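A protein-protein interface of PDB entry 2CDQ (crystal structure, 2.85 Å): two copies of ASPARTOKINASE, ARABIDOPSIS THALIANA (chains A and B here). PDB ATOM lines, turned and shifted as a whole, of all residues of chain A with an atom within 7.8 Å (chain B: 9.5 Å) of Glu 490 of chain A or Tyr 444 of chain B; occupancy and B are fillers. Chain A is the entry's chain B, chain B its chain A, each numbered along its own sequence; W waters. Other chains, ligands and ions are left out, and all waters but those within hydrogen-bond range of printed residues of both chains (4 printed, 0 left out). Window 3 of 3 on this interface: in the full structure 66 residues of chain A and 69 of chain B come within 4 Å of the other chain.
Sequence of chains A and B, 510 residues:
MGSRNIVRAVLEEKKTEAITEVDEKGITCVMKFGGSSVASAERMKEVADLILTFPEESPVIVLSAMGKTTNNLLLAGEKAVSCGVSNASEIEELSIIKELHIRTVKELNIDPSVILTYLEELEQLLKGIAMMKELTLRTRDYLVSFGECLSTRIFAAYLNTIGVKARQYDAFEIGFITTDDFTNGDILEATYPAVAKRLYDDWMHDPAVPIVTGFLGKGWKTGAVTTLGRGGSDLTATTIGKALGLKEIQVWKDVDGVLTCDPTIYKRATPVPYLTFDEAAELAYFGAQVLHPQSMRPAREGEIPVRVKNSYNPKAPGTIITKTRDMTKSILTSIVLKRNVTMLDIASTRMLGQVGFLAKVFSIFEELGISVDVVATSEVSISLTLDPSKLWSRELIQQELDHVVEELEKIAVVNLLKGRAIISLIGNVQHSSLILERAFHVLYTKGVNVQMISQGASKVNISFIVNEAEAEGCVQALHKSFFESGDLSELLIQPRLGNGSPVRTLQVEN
O of Gln 430 of chain A lies within hydrogen-bond range of ND2 of Asn 449 of chain B (2.8 Å). ND1 of His 441 of chain B sits at hydrogen-bond distance from OE2 of Glu 437 of chain A, at 2.7 Å. The side-chain hydroxyl (OG) of Ser 433 of chain A sits at hydrogen-bond distance from the backbone carbonyl oxygen (O) of Val 448 of chain B (2.6 Å). The side-chain amide oxygen of Asn 449 of chain B is in hydrogen-bond range of the backbone NH of Ser 433 of chain A (3.4 Å).
The backbone carbonyl oxygen (O) of Leu 443 of chain B sits at hydrogen-bond distance from the backbone NH (N) of Val 448 of chain B, at 2.8 Å. O of His 441 of chain B is in hydrogen-bond range of OG1 of Thr 445 of chain B (2.9 Å).
Among the printed residues, pairs that only touch across the chains: Leu 491 of chain A with Tyr 444 of chain B (3.6 Å), Glu 437 of chain A with Glu 437 of chain B (3.7 Å), Ser 432 of chain A with Asn 449 of chain B (3.7 Å), Ser 433 of chain A with Tyr 444 of chain B (3.7 Å), Leu 492 of chain A with Tyr 444 of chain B (3.7 Å), Glu 490 of chain A with Tyr 444 of chain B (3.8 Å), Glu 437 of chain A with Phe 440 of chain B (3.8 Å), Ser 433 of chain A with Phe 440 of chain B (3.8 Å), Ser 433 of chain A with Leu 443 of chain B (3.8 Å), Glu 437 of chain A with Tyr 444 of chain B (3.8 Å) and Leu 434 of chain A with Tyr 444 of chain B (3.99 Å).
Glu 490 of chain A touches one residue of chain B. Of the printed residues of chain A, Tyr 444 of chain B touches Ser 433, Leu 434, Glu 437, Glu 490, Leu 491 and Leu 492. No residue of chain B comes within 4 Å of Leu 488 of chain A. No residue of chain B comes within 4 Å of Ser 489 of chain A. Of the printed residues of chain A, His 441 of chain B touches Glu 437 (2.7 Å). Printed residues of chain B within 4 Å of Ser 433 of chain A: Phe 440 (3.8 Å), Leu 443 (3.8 Å), Tyr 444 (3.7 Å), Val 448 (2.6 Å) and Asn 449 (3.4 Å). Of the printed residues of chain A, Val 448 of chain B touches Ser 433 (2.6 Å). Of the printed residues of chain A, Leu 443 of chain B touches Ser 433. Printed residues of chain B within 4 Å of Glu 437 of chain A: Glu 437 (3.7 Å), Phe 440 (3.8 Å), His 441 (2.7 Å) and Tyr 444 (3.8 Å). The nearest printed residue of chain A that does not touch His 441 of chain B is Ser 433 of chain A (5.2 Å).
Hydrophobic or aromatic side chains of chain B that line the printed part of chain A: Phe 440, His 441, Leu 443 and Tyr 444. Among the printed residues, 15 pairs touch across the chains.
Glu 437 of chain B touches its own counterpart, Glu 437 of chain A. Positions printed for both chains: 437 and 438.
Water W1 lies within hydrogen-bond range of N of Val 450 of chain B (2.8 Å), OG of Ser 433 of chain A (2.8 Å) and OG of Ser 432 of chain A (3.0 Å). Water W2 lies within hydrogen-bond range of the side-chain carboxylate (OE2) of Glu 437 of chain A and a ring nitrogen (ND1) of His 441 of chain B. Water W4 lies within hydrogen-bond range of the backbone NH of Leu 434 of chain A (2.9 Å), the side-chain amide oxygen of Asn 449 of chain B (3.1 Å) and the backbone NH of Ser 433 of chain A (3.2 Å). Water W3 bridges OE2 of Glu 437 of chain B (3.3 Å) and OE2 of Glu 437 of chain A (3.5 Å).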
ATOM      1  N   ILE A 331      23.455  17.184   5.173  1.00  0.00           N
ATOM      2  CA  ILE A 331      23.593  17.288   3.720  1.00  0.00           C
ATOM      3  C   ILE A 331      24.054  15.920   3.173  1.00  0.00           C
ATOM      4  O   ILE A 331      23.213  15.116   2.771  1.00  0.00           O
ATOM      5  CB  ILE A 331      24.512  18.484   3.307  1.00  0.00           C
ATOM      6  CG1 ILE A 331      23.778  19.814   3.480  1.00  0.00           C
ATOM      7  CG2 ILE A 331      24.954  18.398   1.861  1.00  0.00           C
ATOM      8  CD1 ILE A 331      23.924  20.433   4.855  1.00  0.00           C
ATOM      9  N   GLN A 430      16.407  15.288   0.837  1.00  0.00           N
ATOM     10  CA  GLN A 430      15.813  16.611   0.713  1.00  0.00           C
ATOM     11  C   GLN A 430      16.746  17.610   0.018  1.00  0.00           C
ATOM     12  O   GLN A 430      16.313  18.676  -0.417  1.00  0.00           O
ATOM     13  CB  GLN A 430      15.395  17.134   2.090  1.00  0.00           C
ATOM     14  CG  GLN A 430      14.084  17.918   2.087  1.00  0.00           C
ATOM     15  CD  GLN A 430      12.854  17.043   2.329  1.00  0.00           C
ATOM     16  OE1 GLN A 430      11.890  17.477   2.971  1.00  0.00           O
ATOM     17  NE2 GLN A 430      12.882  15.809   1.824  1.00  0.00           N
ATOM     18  N   HIS A 431      18.023  17.265  -0.089  1.00  0.00           N
ATOM     19  CA  HIS A 431      18.982  18.134  -0.764  1.00  0.00           C
ATOM     20  C   HIS A 431      19.671  17.425  -1.927  1.00  0.00           C
ATOM     21  O   HIS A 431      20.822  17.723  -2.264  1.00  0.00           O
ATOM     22  CB  HIS A 431      20.006  18.672   0.233  1.00  0.00           C
ATOM     23  CG  HIS A 431      19.390  19.339   1.420  1.00  0.00           C
ATOM     24  ND1 HIS A 431      18.607  20.471   1.316  1.00  0.00           N
ATOM     25  CD2 HIS A 431      19.439  19.034   2.739  1.00  0.00           C
ATOM     26  CE1 HIS A 431      18.202  20.834   2.519  1.00  0.00           C
ATOM     27  NE2 HIS A 431      18.695  19.980   3.400  1.00  0.00           N
ATOM     28  N   SER A 432      18.940  16.498  -2.541  1.00  0.00           N
ATOM     29  CA  SER A 432      19.437  15.699  -3.649  1.00  0.00           C
ATOM     30  C   SER A 432      20.077  16.552  -4.756  1.00  0.00           C
ATOM     31  O   SER A 432      21.234  16.332  -5.118  1.00  0.00           O
ATOM     32  CB  SER A 432      18.313  14.823  -4.205  1.00  0.00           C
ATOM     33  OG  SER A 432      18.695  14.243  -5.434  1.00  0.00           O
ATOM     34  N   SER A 433      19.338  17.533  -5.270  1.00  0.00           N
ATOM     35  CA  SER A 433      19.853  18.375  -6.348  1.00  0.00           C
ATOM     36  C   SER A 433      21.131  19.093  -5.936  1.00  0.00           C
ATOM     37  O   SER A 433      22.077  19.180  -6.725  1.00  0.00           O
ATOM     38  CB  SER A 433      18.803  19.370  -6.824  1.00  0.00           C
ATOM     39  OG  SER A 433      17.682  18.686  -7.346  1.00  0.00           O
ATOM     40  N   LEU A 434      21.156  19.586  -4.700  1.00  0.00           N
ATOM     41  CA  LEU A 434      22.357  20.184  -4.117  1.00  0.00           C
ATOM     42  C   LEU A 434      23.531  19.190  -4.136  1.00  0.00           C
ATOM     43  O   LEU A 434      24.586  19.486  -4.705  1.00  0.00           O
ATOM     44  CB  LEU A 434      22.042  20.710  -2.710  1.00  0.00           C
ATOM     45  CG  LEU A 434      23.046  21.178  -1.645  1.00  0.00           C
ATOM     46  CD1 LEU A 434      24.398  21.626  -2.192  1.00  0.00           C
ATOM     47  CD2 LEU A 434      22.407  22.309  -0.845  1.00  0.00           C
ATOM     48  N   ILE A 435      23.324  18.011  -3.546  1.00  0.00           N
ATOM     49  CA  ILE A 435      24.303  16.914  -3.587  1.00  0.00           C
ATOM     50  C   ILE A 435      24.823  16.703  -5.013  1.00  0.00           C
ATOM     51  O   ILE A 435      26.030  16.765  -5.246  1.00  0.00           O
ATOM     52  CB  ILE A 435      23.716  15.545  -3.080  1.00  0.00           C
ATOM     53  CG1 ILE A 435      22.970  15.661  -1.738  1.00  0.00           C
ATOM     54  CG2 ILE A 435      24.799  14.467  -3.025  1.00  0.00           C
ATOM     55  CD1 ILE A 435      23.698  16.420  -0.660  1.00  0.00           C
ATOM     56  N   GLU A 437      24.546  18.394  -7.992  1.00  0.00           N
ATOM     57  CA  GLU A 437      25.244  19.511  -8.646  1.00  0.00           C
ATOM     58  C   GLU A 437      26.705  19.570  -8.203  1.00  0.00           C
ATOM     59  O   GLU A 437      27.615  19.597  -9.034  1.00  0.00           O
ATOM     60  CB  GLU A 437      24.577  20.856  -8.361  1.00  0.00           C
ATOM     61  CG  GLU A 437      25.367  22.022  -8.960  1.00  0.00           C
ATOM     62  CD  GLU A 437      24.879  23.386  -8.528  1.00  0.00           C
ATOM     63  OE1 GLU A 437      24.045  23.485  -7.597  1.00  0.00           O
ATOM     64  OE2 GLU A 437      25.343  24.371  -9.131  1.00  0.00           O
ATOM     65  N   ARG A 438      26.914  19.584  -6.888  1.00  0.00           N
ATOM     66  CA  ARG A 438      28.253  19.625  -6.322  1.00  0.00           C
ATOM     67  C   ARG A 438      29.077  18.424  -6.785  1.00  0.00           C
ATOM     68  O   ARG A 438      30.195  18.593  -7.276  1.00  0.00           O
ATOM     69  CB  ARG A 438      28.184  19.688  -4.798  1.00  0.00           C
ATOM     70  CG  ARG A 438      29.460  20.178  -4.144  1.00  0.00           C
ATOM     71  CD  ARG A 438      29.209  20.506  -2.690  1.00  0.00           C
ATOM     72  NE  ARG A 438      30.389  21.030  -2.004  1.00  0.00           N
ATOM     73  CZ  ARG A 438      30.767  22.310  -2.003  1.00  0.00           C
ATOM     74  NH1 ARG A 438      30.080  23.231  -2.674  1.00  0.00           N
ATOM     75  NH2 ARG A 438      31.852  22.670  -1.329  1.00  0.00           N
ATOM     76  N   SER A 481      35.232  17.969  -0.978  1.00  0.00           N
ATOM     77  CA  SER A 481      34.161  18.891  -1.366  1.00  0.00           C
ATOM     78  C   SER A 481      32.975  18.893  -0.402  1.00  0.00           C
ATOM     79  O   SER A 481      32.321  19.920  -0.222  1.00  0.00           O
ATOM     80  CB  SER A 481      33.677  18.561  -2.781  1.00  0.00           C
ATOM     81  OG  SER A 481      32.802  19.556  -3.291  1.00  0.00           O
ATOM     82  N   SER A 485      34.934  21.244   3.304  1.00  0.00           N
ATOM     83  CA  SER A 485      34.724  22.605   2.796  1.00  0.00           C
ATOM     84  C   SER A 485      33.905  23.475   3.760  1.00  0.00           C
ATOM     85  O   SER A 485      33.289  24.460   3.347  1.00  0.00           O
ATOM     86  CB  SER A 485      34.063  22.567   1.413  1.00  0.00           C
ATOM     87  OG  SER A 485      34.857  21.845   0.490  1.00  0.00           O
ATOM     88  N   GLY A 486      33.912  23.112   5.042  1.00  0.00           N
ATOM     89  CA  GLY A 486      33.144  23.830   6.058  1.00  0.00           C
ATOM     90  C   GLY A 486      31.662  23.491   6.032  1.00  0.00           C
ATOM     91  O   GLY A 486      31.253  22.515   5.393  1.00  0.00           O
ATOM     92  N   ASP A 487      30.856  24.293   6.731  1.00  0.00           N
ATOM     93  CA  ASP A 487      29.409  24.073   6.800  1.00  0.00           C
ATOM     94  C   ASP A 487      28.736  24.392   5.464  1.00  0.00           C
ATOM     95  O   ASP A 487      28.804  25.522   4.966  1.00  0.00           O
ATOM     96  CB  ASP A 487      28.775  24.887   7.937  1.00  0.00           C
ATOM     97  CG  ASP A 487      27.303  24.534   8.174  1.00  0.00           C
ATOM     98  OD1 ASP A 487      26.614  24.080   7.231  1.00  0.00           O
ATOM     99  OD2 ASP A 487      26.827  24.722   9.315  1.00  0.00           O
ATOM    100  N   LEU A 488      28.085  23.380   4.896  1.00  0.00           N
ATOM    101  CA  LEU A 488      27.445  23.516   3.592  1.00  0.00           C
ATOM    102  C   LEU A 488      26.020  24.060   3.694  1.00  0.00           C
ATOM    103  O   LEU A 488      25.039  23.316   3.592  1.00  0.00           O
ATOM    104  CB  LEU A 488      27.487  22.190   2.823  1.00  0.00           C
ATOM    105  CG  LEU A 488      28.849  21.725   2.300  1.00  0.00           C
ATOM    106  CD1 LEU A 488      28.680  20.400   1.593  1.00  0.00           C
ATOM    107  CD2 LEU A 488      29.497  22.757   1.374  1.00  0.00           C
ATOM    108  N   SER A 489      25.917  25.367   3.912  1.00  0.00           N
ATOM    109  CA  SER A 489      24.627  26.038   3.900  1.00  0.00           C
ATOM    110  C   SER A 489      24.660  27.280   3.019  1.00  0.00           C
ATOM    111  O   SER A 489      24.800  28.407   3.496  1.00  0.00           O
ATOM    112  CB  SER A 489      24.149  26.329   5.320  1.00  0.00           C
ATOM    113  OG  SER A 489      23.801  25.111   5.957  1.00  0.00           O
ATOM    114  N   GLU A 490      24.589  27.028   1.715  1.00  0.00           N
ATOM    115  CA  GLU A 490      24.291  28.044   0.716  1.00  0.00           C
ATOM    116  C   GLU A 490      22.791  27.930   0.480  1.00  0.00           C
ATOM    117  O   GLU A 490      22.155  28.858  -0.030  1.00  0.00           O
ATOM    118  CB  GLU A 490      25.046  27.796  -0.596  1.00  0.00           C
ATOM    119  CG  GLU A 490      26.378  27.050  -0.471  1.00  0.00           C
ATOM    120  CD  GLU A 490      26.226  25.543  -0.650  1.00  0.00           C
ATOM    121  OE1 GLU A 490      26.453  24.796   0.325  1.00  0.00           O
ATOM    122  OE2 GLU A 490      25.874  25.103  -1.764  1.00  0.00           O
ATOM    123  N   LEU A 491      22.264  26.754   0.837  1.00  0.00           N
ATOM    124  CA  LEU A 491      20.831  26.452   0.989  1.00  0.00           C
ATOM    125  C   LEU A 491      19.885  27.662   0.936  1.00  0.00           C
ATOM    126  O   LEU A 491      19.952  28.550   1.794  1.00  0.00           O
ATOM    127  CB  LEU A 491      20.640  25.701   2.313  1.00  0.00           C
ATOM    128  CG  LEU A 491      19.689  24.508   2.386  1.00  0.00           C
ATOM    129  CD1 LEU A 491      20.151  23.574   3.486  1.00  0.00           C
ATOM    130  CD2 LEU A 491      18.250  24.954   2.620  1.00  0.00           C
ATOM    131  N   LEU A 492      19.001  27.676  -0.065  1.00  0.00           N
ATOM    132  CA  LEU A 492      18.081  28.802  -0.302  1.00  0.00           C
ATOM    133  C   LEU A 492      16.939  28.891   0.720  1.00  0.00           C
ATOM    134  O   LEU A 492      16.089  27.998   0.797  1.00  0.00           O
ATOM    135  CB  LEU A 492      17.515  28.753  -1.732  1.00  0.00           C
ATOM    136  CG  LEU A 492      18.457  28.983  -2.924  1.00  0.00           C
ATOM    137  CD1 LEU A 492      17.816  28.494  -4.215  1.00  0.00           C
ATOM    138  CD2 LEU A 492      18.878  30.451  -3.050  1.00  0.00           C
ATOM    139  N   ILE A 493      16.935  29.974   1.501  1.00  0.00           N
ATOM    140  CA  ILE A 493      15.897  30.228   2.509  1.00  0.00           C
ATOM    141  C   ILE A 493      15.160  31.539   2.187  1.00  0.00           C
ATOM    142  O   ILE A 493      14.905  31.836   1.018  1.00  0.00           O
ATOM    143  CB  ILE A 493      16.457  30.259   3.981  1.00  0.00           C
ATOM    144  CG1 ILE A 493      17.924  29.806   4.069  1.00  0.00           C
ATOM    145  CG2 ILE A 493      15.556  29.457   4.925  1.00  0.00           C
ATOM    146  CD1 ILE A 493      18.942  30.949   4.012  1.00  0.00           C
ATOM    147  N   LEU B 436      25.340  17.128 -16.327  1.00  0.00           N
ATOM    148  CA  LEU B 436      24.689  16.815 -15.060  1.00  0.00           C
ATOM    149  C   LEU B 436      24.844  17.889 -14.002  1.00  0.00           C
ATOM    150  O   LEU B 436      23.894  18.162 -13.269  1.00  0.00           O
ATOM    151  CB  LEU B 436      25.127  15.444 -14.535  1.00  0.00           C
ATOM    152  CG  LEU B 436      24.214  14.251 -14.853  1.00  0.00           C
ATOM    153  CD1 LEU B 436      23.080  14.600 -15.806  1.00  0.00           C
ATOM    154  CD2 LEU B 436      25.016  13.090 -15.398  1.00  0.00           C
ATOM    155  N   GLU B 437      26.027  18.499 -13.926  1.00  0.00           N
ATOM    156  CA  GLU B 437      26.236  19.652 -13.040  1.00  0.00           C
ATOM    157  C   GLU B 437      25.215  20.741 -13.363  1.00  0.00           C
ATOM    158  O   GLU B 437      24.539  21.258 -12.469  1.00  0.00           O
ATOM    159  CB  GLU B 437      27.658  20.222 -13.160  1.00  0.00           C
ATOM    160  CG  GLU B 437      27.901  21.409 -12.209  1.00  0.00           C
ATOM    161  CD  GLU B 437      29.185  22.195 -12.474  1.00  0.00           C
ATOM    162  OE1 GLU B 437      30.005  21.783 -13.326  1.00  0.00           O
ATOM    163  OE2 GLU B 437      29.377  23.234 -11.807  1.00  0.00           O
ATOM    164  N   ARG B 438      25.099  21.062 -14.650  1.00  0.00           N
ATOM    165  CA  ARG B 438      24.200  22.112 -15.111  1.00  0.00           C
ATOM    166  C   ARG B 438      22.732  21.779 -14.823  1.00  0.00           C
ATOM    167  O   ARG B 438      22.007  22.596 -14.236  1.00  0.00           O
ATOM    168  CB  ARG B 438      24.414  22.371 -16.602  1.00  0.00           C
ATOM    169  CG  ARG B 438      23.889  23.710 -17.073  1.00  0.00           C
ATOM    170  CD  ARG B 438      24.367  24.000 -18.474  1.00  0.00           C
ATOM    171  NE  ARG B 438      23.966  25.323 -18.953  1.00  0.00           N
ATOM    172  CZ  ARG B 438      24.618  26.457 -18.693  1.00  0.00           C
ATOM    173  NH1 ARG B 438      25.706  26.462 -17.926  1.00  0.00           N
ATOM    174  NH2 ARG B 438      24.172  27.599 -19.199  1.00  0.00           N
ATOM    175  N   ALA B 439      22.319  20.571 -15.221  1.00  0.00           N
ATOM    176  CA  ALA B 439      20.949  20.094 -15.042  1.00  0.00           C
ATOM    177  C   ALA B 439      20.495  20.225 -13.589  1.00  0.00           C
ATOM    178  O   ALA B 439      19.494  20.894 -13.297  1.00  0.00           O
ATOM    179  CB  ALA B 439      20.831  18.659 -15.507  1.00  0.00           C
ATOM    180  N   PHE B 440      21.251  19.609 -12.683  1.00  0.00           N
ATOM    181  CA  PHE B 440      20.920  19.643 -11.266  1.00  0.00           C
ATOM    182  C   PHE B 440      21.037  21.033 -10.665  1.00  0.00           C
ATOM    183  O   PHE B 440      20.305  21.360  -9.723  1.00  0.00           O
ATOM    184  CB  PHE B 440      21.739  18.622 -10.487  1.00  0.00           C
ATOM    185  CG  PHE B 440      21.304  17.213 -10.732  1.00  0.00           C
ATOM    186  CD1 PHE B 440      21.991  16.406 -11.635  1.00  0.00           C
ATOM    187  CD2 PHE B 440      20.181  16.699 -10.085  1.00  0.00           C
ATOM    188  CE1 PHE B 440      21.577  15.105 -11.875  1.00  0.00           C
ATOM    189  CE2 PHE B 440      19.761  15.399 -10.318  1.00  0.00           C
ATOM    190  CZ  PHE B 440      20.456  14.598 -11.212  1.00  0.00           C
ATOM    191  N   HIS B 441      21.925  21.859 -11.215  1.00  0.00           N
ATOM    192  CA  HIS B 441      21.969  23.248 -10.793  1.00  0.00           C
ATOM    193  C   HIS B 441      20.623  23.900 -11.080  1.00  0.00           C
ATOM    194  O   HIS B 441      20.061  24.580 -10.216  1.00  0.00           O
ATOM    195  CB  HIS B 441      23.075  24.034 -11.480  1.00  0.00           C
ATOM    196  CG  HIS B 441      23.023  25.497 -11.174  1.00  0.00           C
ATOM    197  ND1 HIS B 441      23.279  26.003  -9.915  1.00  0.00           N
ATOM    198  CD2 HIS B 441      22.700  26.559 -11.950  1.00  0.00           C
ATOM    199  CE1 HIS B 441      23.136  27.316  -9.934  1.00  0.00           C
ATOM    200  NE2 HIS B 441      22.785  27.679 -11.157  1.00  0.00           N
ATOM    201  N   VAL B 442      20.108  23.673 -12.289  1.00  0.00           N
ATOM    202  CA  VAL B 442      18.806  24.213 -12.687  1.00  0.00           C
ATOM    203  C   VAL B 442      17.711  23.716 -11.742  1.00  0.00           C
ATOM    204  O   VAL B 442      16.928  24.512 -11.217  1.00  0.00           O
ATOM    205  CB  VAL B 442      18.465  23.874 -14.161  1.00  0.00           C
ATOM    206  CG1 VAL B 442      17.032  24.231 -14.479  1.00  0.00           C
ATOM    207  CG2 VAL B 442      19.405  24.602 -15.102  1.00  0.00           C
ATOM    208  N   LEU B 443      17.683  22.405 -11.513  1.00  0.00           N
ATOM    209  CA  LEU B 443      16.676  21.806 -10.652  1.00  0.00           C
ATOM    210  C   LEU B 443      16.750  22.327  -9.213  1.00  0.00           C
ATOM    211  O   LEU B 443      15.710  22.569  -8.591  1.00  0.00           O
ATOM    212  CB  LEU B 443      16.764  20.282 -10.695  1.00  0.00           C
ATOM    213  CG  LEU B 443      16.392  19.641 -12.032  1.00  0.00           C
ATOM    214  CD1 LEU B 443      16.573  18.146 -11.955  1.00  0.00           C
ATOM    215  CD2 LEU B 443      14.957  19.967 -12.433  1.00  0.00           C
ATOM    216  N   TYR B 444      17.973  22.508  -8.703  1.00  0.00           N
ATOM    217  CA  TYR B 444      18.203  23.061  -7.359  1.00  0.00           C
ATOM    218  C   TYR B 444      17.668  24.489  -7.243  1.00  0.00           C
ATOM    219  O   TYR B 444      17.030  24.840  -6.244  1.00  0.00           O
ATOM    220  CB  TYR B 444      19.693  22.997  -6.997  1.00  0.00           C
ATOM    221  CG  TYR B 444      20.125  23.874  -5.833  1.00  0.00           C
ATOM    222  CD1 TYR B 444      19.779  23.550  -4.522  1.00  0.00           C
ATOM    223  CD2 TYR B 444      20.903  25.014  -6.047  1.00  0.00           C
ATOM    224  CE1 TYR B 444      20.177  24.350  -3.456  1.00  0.00           C
ATOM    225  CE2 TYR B 444      21.308  25.821  -4.989  1.00  0.00           C
ATOM    226  CZ  TYR B 444      20.941  25.484  -3.694  1.00  0.00           C
ATOM    227  OH  TYR B 444      21.337  26.282  -2.635  1.00  0.00           O
ATOM    228  N   THR B 445      17.928  25.295  -8.275  1.00  0.00           N
ATOM    229  CA  THR B 445      17.422  26.672  -8.376  1.00  0.00           C
ATOM    230  C   THR B 445      15.895  26.725  -8.209  1.00  0.00           C
ATOM    231  O   THR B 445      15.358  27.597  -7.514  1.00  0.00           O
ATOM    232  CB  THR B 445      17.843  27.307  -9.729  1.00  0.00           C
ATOM    233  OG1 THR B 445      19.273  27.350  -9.807  1.00  0.00           O
ATOM    234  CG2 THR B 445      17.290  28.717  -9.892  1.00  0.00           C
ATOM    235  N   LYS B 446      15.213  25.770  -8.836  1.00  0.00           N
ATOM    236  CA  LYS B 446      13.764  25.679  -8.785  1.00  0.00           C
ATOM    237  C   LYS B 446      13.272  25.029  -7.500  1.00  0.00           C
ATOM    238  O   LYS B 446      12.086  25.100  -7.193  1.00  0.00           O
ATOM    239  CB  LYS B 446      13.241  24.889  -9.983  1.00  0.00           C
ATOM    240  CG  LYS B 446      13.536  25.516 -11.346  1.00  0.00           C
ATOM    241  CD  LYS B 446      12.985  24.656 -12.484  1.00  0.00           C
ATOM    242  CE  LYS B 446      11.463  24.703 -12.567  1.00  0.00           C
ATOM    243  NZ  LYS B 446      10.992  26.062 -12.953  1.00  0.00           N
ATOM    244  N   GLY B 447      14.171  24.393  -6.753  1.00  0.00           N
ATOM    245  CA  GLY B 447      13.784  23.679  -5.536  1.00  0.00           C
ATOM    246  C   GLY B 447      13.172  22.323  -5.842  1.00  0.00           C
ATOM    247  O   GLY B 447      12.356  21.808  -5.073  1.00  0.00           O
ATOM    248  N   VAL B 448      13.575  21.744  -6.970  1.00  0.00           N
ATOM    249  CA  VAL B 448      13.067  20.445  -7.407  1.00  0.00           C
ATOM    250  C   VAL B 448      14.059  19.335  -7.086  1.00  0.00           C
ATOM    251  O   VAL B 448      15.242  19.444  -7.408  1.00  0.00           O
ATOM    252  CB  VAL B 448      12.783  20.431  -8.918  1.00  0.00           C
ATOM    253  CG1 VAL B 448      12.247  19.079  -9.349  1.00  0.00           C
ATOM    254  CG2 VAL B 448      11.807  21.535  -9.287  1.00  0.00           C
ATOM    255  N   ASN B 449      13.566  18.277  -6.444  1.00  0.00           N
ATOM    256  CA  ASN B 449      14.356  17.074  -6.197  1.00  0.00           C
ATOM    257  C   ASN B 449      13.873  15.907  -7.038  1.00  0.00           C
ATOM    258  O   ASN B 449      12.697  15.551  -7.003  1.00  0.00           O
ATOM    259  CB  ASN B 449      14.343  16.693  -4.716  1.00  0.00           C
ATOM    260  CG  ASN B 449      15.206  17.611  -3.868  1.00  0.00           C
ATOM    261  OD1 ASN B 449      16.171  18.216  -4.351  1.00  0.00           O
ATOM    262  ND2 ASN B 449      14.867  17.711  -2.588  1.00  0.00           N
ATOM    263  N   VAL B 450      14.789  15.331  -7.803  1.00  0.00           N
ATOM    264  CA  VAL B 450      14.504  14.170  -8.628  1.00  0.00           C
ATOM    265  C   VAL B 450      14.306  12.965  -7.727  1.00  0.00           C
ATOM    266  O   VAL B 450      15.140  12.687  -6.862  1.00  0.00           O
ATOM    267  CB  VAL B 450      15.649  13.915  -9.631  1.00  0.00           C
ATOM    268  CG1 VAL B 450      15.464  12.592 -10.342  1.00  0.00           C
ATOM    269  CG2 VAL B 450      15.732  15.059 -10.640  1.00  0.00           C
ATOM    270  N   CYS B 474       9.911  22.349 -15.490  1.00  0.00           N
ATOM    271  CA  CYS B 474      11.290  21.861 -15.442  1.00  0.00           C
ATOM    272  C   CYS B 474      11.880  21.753 -16.840  1.00  0.00           C
ATOM    273  O   CYS B 474      13.016  22.170 -17.067  1.00  0.00           O
ATOM    274  CB  CYS B 474      11.378  20.504 -14.744  1.00  0.00           C
ATOM    275  SG  CYS B 474      11.248  20.564 -12.954  1.00  0.00           S
ATOM    276  N   ALA B 477      12.744  25.192 -18.124  1.00  0.00           N
ATOM    277  CA  ALA B 477      13.954  25.658 -17.450  1.00  0.00           C
ATOM    278  C   ALA B 477      15.216  24.987 -18.018  1.00  0.00           C
ATOM    279  O   ALA B 477      16.197  25.664 -18.346  1.00  0.00           O
ATOM    280  CB  ALA B 477      13.845  25.427 -15.959  1.00  0.00           C
ATOM    281  N   LEU B 478      15.175  23.662 -18.153  1.00  0.00           N
ATOM    282  CA  LEU B 478      16.303  22.907 -18.685  1.00  0.00           C
ATOM    283  C   LEU B 478      16.654  23.349 -20.108  1.00  0.00           C
ATOM    284  O   LEU B 478      17.830  23.519 -20.443  1.00  0.00           O
ATOM    285  CB  LEU B 478      16.028  21.400 -18.620  1.00  0.00           C
ATOM    286  CG  LEU B 478      16.099  20.738 -17.232  1.00  0.00           C
ATOM    287  CD1 LEU B 478      15.663  19.288 -17.301  1.00  0.00           C
ATOM    288  CD2 LEU B 478      17.493  20.837 -16.600  1.00  0.00           C
HETATM  289  O   HOH W   1      17.506  15.864  -7.677  1.00  0.00           O
HETATM  290  O   HOH W   2      25.163  26.153  -7.005  1.00  0.00           O
HETATM  291  O   HOH W   3      26.614  24.958 -12.334  1.00  0.00           O
HETATM  292  O   HOH W   4      18.515  20.039  -3.546  1.00  0.00           O
